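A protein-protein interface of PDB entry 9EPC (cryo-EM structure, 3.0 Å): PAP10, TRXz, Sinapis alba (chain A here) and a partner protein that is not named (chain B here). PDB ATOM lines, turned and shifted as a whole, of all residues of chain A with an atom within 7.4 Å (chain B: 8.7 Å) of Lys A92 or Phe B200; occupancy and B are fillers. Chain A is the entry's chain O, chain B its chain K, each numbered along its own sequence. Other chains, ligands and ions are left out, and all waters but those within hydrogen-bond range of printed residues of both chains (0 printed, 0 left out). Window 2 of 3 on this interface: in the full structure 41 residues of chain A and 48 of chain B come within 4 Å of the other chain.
O of Gly B203 is in hydrogen-bond range of NE2 of Gln A88 (3.3 Å). N of Met B205 is in hydrogen-bond range of OE1 of Gln A88, 3.1 Å away.
Leu A87 touches Met B205. Lys B204 touches Gln A88. Val A91 touches Phe B200. Val A91 touches Met B205. Lys A92 touches Phe B200.
Of the printed residues of chain B, Leu A87 touches Met B205 (3.8 Å). Printed residues of chain B within 4 Å of Gln A88: Gly B203, Lys B204 and Met B205. Of the printed residues of chain B, Val A91 touches Phe B200 (3.6 Å) and Met B205 (3.9 Å). Of chain A, only Val A91 and Lys A92 come within 4 Å of Phe B200. Printed residues of chain A within 4 Å of Gly B203: Gln A88 (3.3 Å). Of the printed residues of chain A, Lys B204 touches Gln A88 (3.4 Å). Of the printed residues of chain A, Met B205 touches Leu A87, Gln A88 and Val A91. The nearest residue of chain A that does not touch Phe B200 is Gln A88 (4.7 Å). The nearest printed residue of chain B that does not touch Gln A88 is Phe B200 (4.7 Å).
Of the 11 printed residues of chain B, 4 touch a printed residue of chain A. Hydrophobic or aromatic side chains of chain B that line the printed part of chain A: Phe B200 and Met B205. Printed residues of chain A that touch a printed residue of chain B: Leu A87, Gln A88, Val A91 and Lys A92. Among the printed residues, 7 pairs touch across the chains. Among the printed residues, no Asp or Glu carboxylate lies within 4 Å of a Lys or Arg side-chain nitrogen of the other chain.
The backbone carbonyl oxygen (O) of Val A91 sits at hydrogen-bond distance from the guanidinium group (NH1) of Arg A95 (2.7 Å).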
ATOM      1  N   GLN A  85      24.184  12.552  23.810  1.00  0.00           N
ATOM      2  CA  GLN A  85      24.948  13.780  23.998  1.00  0.00           C
ATOM      3  C   GLN A  85      25.568  14.259  22.694  1.00  0.00           C
ATOM      4  O   GLN A  85      25.546  15.456  22.398  1.00  0.00           O
ATOM      5  CB  GLN A  85      26.035  13.576  25.050  1.00  0.00           C
ATOM      6  CG  GLN A  85      27.036  14.726  25.145  1.00  0.00           C
ATOM      7  CD  GLN A  85      26.406  16.023  25.617  1.00  0.00           C
ATOM      8  OE1 GLN A  85      25.923  16.831  24.813  1.00  0.00           O
ATOM      9  NE2 GLN A  85      26.419  16.236  26.930  1.00  0.00           N
ATOM     10  N   GLU A  86      26.135  13.343  21.907  1.00  0.00           N
ATOM     11  CA  GLU A  86      26.740  13.741  20.642  1.00  0.00           C
ATOM     12  C   GLU A  86      25.702  14.378  19.729  1.00  0.00           C
ATOM     13  O   GLU A  86      26.019  15.284  18.950  1.00  0.00           O
ATOM     14  CB  GLU A  86      27.387  12.539  19.952  1.00  0.00           C
ATOM     15  CG  GLU A  86      28.598  11.982  20.682  1.00  0.00           C
ATOM     16  CD  GLU A  86      29.168  10.748  20.007  1.00  0.00           C
ATOM     17  OE1 GLU A  86      28.512  10.217  19.086  1.00  0.00           O
ATOM     18  OE2 GLU A  86      30.268  10.308  20.398  1.00  0.00           O
ATOM     19  N   LEU A  87      24.450  13.929  19.827  1.00  0.00           N
ATOM     20  CA  LEU A  87      23.369  14.568  19.087  1.00  0.00           C
ATOM     21  C   LEU A  87      23.039  15.943  19.655  1.00  0.00           C
ATOM     22  O   LEU A  87      22.683  16.858  18.903  1.00  0.00           O
ATOM     23  CB  LEU A  87      22.132  13.674  19.096  1.00  0.00           C
ATOM     24  CG  LEU A  87      20.960  14.152  18.247  1.00  0.00           C
ATOM     25  CD1 LEU A  87      21.393  14.311  16.804  1.00  0.00           C
ATOM     26  CD2 LEU A  87      19.804  13.183  18.359  1.00  0.00           C
ATOM     27  N   GLN A  88      23.154  16.115  20.975  1.00  0.00           N
ATOM     28  CA  GLN A  88      22.742  17.375  21.589  1.00  0.00           C
ATOM     29  C   GLN A  88      23.608  18.533  21.118  1.00  0.00           C
ATOM     30  O   GLN A  88      23.094  19.569  20.683  1.00  0.00           O
ATOM     31  CB  GLN A  88      22.791  17.270  23.111  1.00  0.00           C
ATOM     32  CG  GLN A  88      21.618  16.539  23.713  1.00  0.00           C
ATOM     33  CD  GLN A  88      21.497  16.778  25.201  1.00  0.00           C
ATOM     34  OE1 GLN A  88      20.669  16.164  25.873  1.00  0.00           O
ATOM     35  NE2 GLN A  88      22.321  17.677  25.727  1.00  0.00           N
ATOM     36  N   ASP A  89      24.929  18.380  21.205  1.00  0.00           N
ATOM     37  CA  ASP A  89      25.815  19.456  20.784  1.00  0.00           C
ATOM     38  C   ASP A  89      25.728  19.689  19.285  1.00  0.00           C
ATOM     39  O   ASP A  89      25.960  20.809  18.817  1.00  0.00           O
ATOM     40  CB  ASP A  89      27.259  19.146  21.185  1.00  0.00           C
ATOM     41  CG  ASP A  89      27.482  19.242  22.681  1.00  0.00           C
ATOM     42  OD1 ASP A  89      26.617  19.814  23.376  1.00  0.00           O
ATOM     43  OD2 ASP A  89      28.490  18.773  23.249  1.00  0.00           O
ATOM     44  N   LEU A  90      25.398  18.648  18.521  1.00  0.00           N
ATOM     45  CA  LEU A  90      25.157  18.826  17.096  1.00  0.00           C
ATOM     46  C   LEU A  90      23.960  19.736  16.854  1.00  0.00           C
ATOM     47  O   LEU A  90      24.002  20.610  15.981  1.00  0.00           O
ATOM     48  CB  LEU A  90      24.946  17.469  16.433  1.00  0.00           C
ATOM     49  CG  LEU A  90      24.902  17.475  14.910  1.00  0.00           C
ATOM     50  CD1 LEU A  90      26.195  18.041  14.356  1.00  0.00           C
ATOM     51  CD2 LEU A  90      24.668  16.071  14.397  1.00  0.00           C
ATOM     52  N   VAL A  91      22.881  19.544  17.615  1.00  0.00           N
ATOM     53  CA  VAL A  91      21.726  20.425  17.491  1.00  0.00           C
ATOM     54  C   VAL A  91      22.042  21.805  18.050  1.00  0.00           C
ATOM     55  O   VAL A  91      21.689  22.828  17.450  1.00  0.00           O
ATOM     56  CB  VAL A  91      20.499  19.804  18.181  1.00  0.00           C
ATOM     57  CG1 VAL A  91      19.310  20.739  18.076  1.00  0.00           C
ATOM     58  CG2 VAL A  91      20.171  18.459  17.564  1.00  0.00           C
ATOM     59  N   LYS A  92      22.709  21.861  19.206  1.00  0.00           N
ATOM     60  CA  LYS A  92      23.075  23.151  19.780  1.00  0.00           C
ATOM     61  C   LYS A  92      24.058  23.899  18.891  1.00  0.00           C
ATOM     62  O   LYS A  92      23.963  25.124  18.754  1.00  0.00           O
ATOM     63  CB  LYS A  92      23.666  22.965  21.176  1.00  0.00           C
ATOM     64  CG  LYS A  92      22.712  22.353  22.180  1.00  0.00           C
ATOM     65  CD  LYS A  92      22.776  23.081  23.509  1.00  0.00           C
ATOM     66  CE  LYS A  92      24.194  23.126  24.048  1.00  0.00           C
ATOM     67  NZ  LYS A  92      24.270  23.891  25.322  1.00  0.00           N
ATOM     68  N   GLY A  93      25.003  23.190  18.284  1.00  0.00           N
ATOM     69  CA  GLY A  93      25.941  23.819  17.383  1.00  0.00           C
ATOM     70  C   GLY A  93      25.283  24.251  16.089  1.00  0.00           C
ATOM     71  O   GLY A  93      24.165  23.863  15.751  1.00  0.00           O
ATOM     72  N   GLU A  94      26.009  25.084  15.346  1.00  0.00           N
ATOM     73  CA  GLU A  94      25.516  25.639  14.089  1.00  0.00           C
ATOM     74  C   GLU A  94      25.677  24.604  12.983  1.00  0.00           C
ATOM     75  O   GLU A  94      26.789  24.136  12.714  1.00  0.00           O
ATOM     76  CB  GLU A  94      26.253  26.927  13.737  1.00  0.00           C
ATOM     77  CG  GLU A  94      26.323  27.226  12.238  1.00  0.00           C
ATOM     78  CD  GLU A  94      24.957  27.394  11.589  1.00  0.00           C
ATOM     79  OE1 GLU A  94      24.842  27.131  10.372  1.00  0.00           O
ATOM     80  OE2 GLU A  94      24.006  27.790  12.292  1.00  0.00           O
ATOM     81  N   ARG A  95      24.569  24.248  12.347  1.00  0.00           N
ATOM     82  CA  ARG A  95      24.564  23.349  11.205  1.00  0.00           C
ATOM     83  C   ARG A  95      24.085  24.116   9.983  1.00  0.00           C
ATOM     84  O   ARG A  95      23.056  24.796  10.037  1.00  0.00           O
ATOM     85  CB  ARG A  95      23.662  22.144  11.459  1.00  0.00           C
ATOM     86  CG  ARG A  95      23.623  21.709  12.903  1.00  0.00           C
ATOM     87  CD  ARG A  95      22.386  20.887  13.166  1.00  0.00           C
ATOM     88  NE  ARG A  95      21.177  21.621  12.819  1.00  0.00           N
ATOM     89  CZ  ARG A  95      20.542  22.444  13.641  1.00  0.00           C
ATOM     90  NH1 ARG A  95      20.981  22.670  14.867  1.00  0.00           N
ATOM     91  NH2 ARG A  95      19.438  23.053  13.222  1.00  0.00           N
ATOM     92  N   LYS B 197       8.918  20.983  17.966  1.00  0.00           N
ATOM     93  CA  LYS B 197       9.889  21.993  18.359  1.00  0.00           C
ATOM     94  C   LYS B 197      10.863  21.383  19.354  1.00  0.00           C
ATOM     95  O   LYS B 197      10.444  20.787  20.351  1.00  0.00           O
ATOM     96  CB  LYS B 197       9.205  23.212  18.979  1.00  0.00           C
ATOM     97  CG  LYS B 197      10.140  24.394  19.174  1.00  0.00           C
ATOM     98  CD  LYS B 197       9.582  25.400  20.165  1.00  0.00           C
ATOM     99  CE  LYS B 197       9.599  24.844  21.580  1.00  0.00           C
ATOM    100  NZ  LYS B 197       9.202  25.864  22.587  1.00  0.00           N
ATOM    101  N   ILE B 198      12.150  21.536  19.085  1.00  0.00           N
ATOM    102  CA  ILE B 198      13.194  21.012  19.954  1.00  0.00           C
ATOM    103  C   ILE B 198      13.502  22.041  21.029  1.00  0.00           C
ATOM    104  O   ILE B 198      13.800  23.202  20.725  1.00  0.00           O
ATOM    105  CB  ILE B 198      14.455  20.664  19.150  1.00  0.00           C
ATOM    106  CG1 ILE B 198      14.140  19.589  18.113  1.00  0.00           C
ATOM    107  CG2 ILE B 198      15.562  20.208  20.076  1.00  0.00           C
ATOM    108  CD1 ILE B 198      15.340  19.154  17.328  1.00  0.00           C
ATOM    109  N   LYS B 199      13.432  21.620  22.288  1.00  0.00           N
ATOM    110  CA  LYS B 199      13.702  22.495  23.420  1.00  0.00           C
ATOM    111  C   LYS B 199      14.679  21.813  24.362  1.00  0.00           C
ATOM    112  O   LYS B 199      14.535  20.621  24.654  1.00  0.00           O
ATOM    113  CB  LYS B 199      12.411  22.855  24.156  1.00  0.00           C
ATOM    114  CG  LYS B 199      11.458  21.688  24.330  1.00  0.00           C
ATOM    115  CD  LYS B 199      10.199  22.111  25.061  1.00  0.00           C
ATOM    116  CE  LYS B 199      10.480  22.384  26.527  1.00  0.00           C
ATOM    117  NZ  LYS B 199      10.939  21.155  27.228  1.00  0.00           N
ATOM    118  N   PHE B 200      15.666  22.567  24.833  1.00  0.00           N
ATOM    119  CA  PHE B 200      16.677  22.054  25.753  1.00  0.00           C
ATOM    120  C   PHE B 200      16.229  22.375  27.172  1.00  0.00           C
ATOM    121  O   PHE B 200      16.447  23.481  27.671  1.00  0.00           O
ATOM    122  CB  PHE B 200      18.038  22.661  25.444  1.00  0.00           C
ATOM    123  CG  PHE B 200      18.457  22.497  24.017  1.00  0.00           C
ATOM    124  CD1 PHE B 200      18.284  21.289  23.369  1.00  0.00           C
ATOM    125  CD2 PHE B 200      19.007  23.555  23.319  1.00  0.00           C
ATOM    126  CE1 PHE B 200      18.663  21.135  22.054  1.00  0.00           C
ATOM    127  CE2 PHE B 200      19.386  23.407  22.003  1.00  0.00           C
ATOM    128  CZ  PHE B 200      19.214  22.196  21.370  1.00  0.00           C
ATOM    129  N   GLU B 201      15.603  21.402  27.825  1.00  0.00           N
ATOM    130  CA  GLU B 201      15.059  21.573  29.164  1.00  0.00           C
ATOM    131  C   GLU B 201      15.875  20.756  30.154  1.00  0.00           C
ATOM    132  O   GLU B 201      16.056  19.549  29.965  1.00  0.00           O
ATOM    133  CB  GLU B 201      13.591  21.149  29.211  1.00  0.00           C
ATOM    134  CG  GLU B 201      12.948  21.287  30.578  1.00  0.00           C
ATOM    135  CD  GLU B 201      11.483  20.903  30.571  1.00  0.00           C
ATOM    136  OE1 GLU B 201      10.999  20.422  29.525  1.00  0.00           O
ATOM    137  OE2 GLU B 201      10.815  21.084  31.610  1.00  0.00           O
ATOM    138  N   ASP B 202      16.358  21.421  31.205  1.00  0.00           N
ATOM    139  CA  ASP B 202      17.123  20.773  32.271  1.00  0.00           C
ATOM    140  C   ASP B 202      18.354  20.059  31.716  1.00  0.00           C
ATOM    141  O   ASP B 202      18.735  18.983  32.181  1.00  0.00           O
ATOM    142  CB  ASP B 202      16.242  19.809  33.070  1.00  0.00           C
ATOM    143  CG  ASP B 202      16.839  19.451  34.415  1.00  0.00           C
ATOM    144  OD1 ASP B 202      16.864  20.324  35.308  1.00  0.00           O
ATOM    145  OD2 ASP B 202      17.286  18.296  34.579  1.00  0.00           O
ATOM    146  N   GLY B 203      18.978  20.659  30.706  1.00  0.00           N
ATOM    147  CA  GLY B 203      20.176  20.108  30.114  1.00  0.00           C
ATOM    148  C   GLY B 203      19.962  18.923  29.199  1.00  0.00           C
ATOM    149  O   GLY B 203      20.940  18.410  28.641  1.00  0.00           O
ATOM    150  N   LYS B 204      18.725  18.472  29.021  1.00  0.00           N
ATOM    151  CA  LYS B 204      18.410  17.347  28.150  1.00  0.00           C
ATOM    152  C   LYS B 204      17.533  17.827  27.004  1.00  0.00           C
ATOM    153  O   LYS B 204      16.532  18.516  27.229  1.00  0.00           O
ATOM    154  CB  LYS B 204      17.705  16.231  28.922  1.00  0.00           C
ATOM    155  CG  LYS B 204      18.528  15.633  30.047  1.00  0.00           C
ATOM    156  CD  LYS B 204      17.849  14.407  30.635  1.00  0.00           C
ATOM    157  CE  LYS B 204      16.461  14.739  31.153  1.00  0.00           C
ATOM    158  NZ  LYS B 204      15.783  13.543  31.723  1.00  0.00           N
ATOM    159  N   MET B 205      17.909  17.464  25.782  1.00  0.00           N
ATOM    160  CA  MET B 205      17.116  17.831  24.618  1.00  0.00           C
ATOM    161  C   MET B 205      15.784  17.094  24.635  1.00  0.00           C
ATOM    162  O   MET B 205      15.732  15.887  24.884  1.00  0.00           O
ATOM    163  CB  MET B 205      17.882  17.516  23.334  1.00  0.00           C
ATOM    164  CG  MET B 205      17.001  17.359  22.108  1.00  0.00           C
ATOM    165  SD  MET B 205      17.896  17.555  20.557  1.00  0.00           S
ATOM    166  CE  MET B 205      19.184  16.331  20.744  1.00  0.00           C
ATOM    167  N   LYS B 206      14.703  17.829  24.383  1.00  0.00           N
ATOM    168  CA  LYS B 206      13.366  17.262  24.308  1.00  0.00           C
ATOM    169  C   LYS B 206      12.653  17.857  23.104  1.00  0.00           C
ATOM    170  O   LYS B 206      13.175  18.741  22.419  1.00  0.00           O
ATOM    171  CB  LYS B 206      12.576  17.517  25.596  1.00  0.00           C
ATOM    172  CG  LYS B 206      13.133  16.809  26.815  1.00  0.00           C
ATOM    173  CD  LYS B 206      12.231  17.004  28.019  1.00  0.00           C
ATOM    174  CE  LYS B 206      12.783  16.287  29.238  1.00  0.00           C
ATOM    175  NZ  LYS B 206      11.896  16.446  30.422  1.00  0.00           N
ATOM    176  N   ALA B 207      11.447  17.362  22.842  1.00  0.00           N
ATOM    177  CA  ALA B 207      10.635  17.850  21.741  1.00  0.00           C
ATOM    178  C   ALA B 207       9.188  17.956  22.193  1.00  0.00           C
ATOM    179  O   ALA B 207       8.760  17.266  23.121  1.00  0.00           O
ATOM    180  CB  ALA B 207      10.736  16.938  20.513  1.00  0.00           C
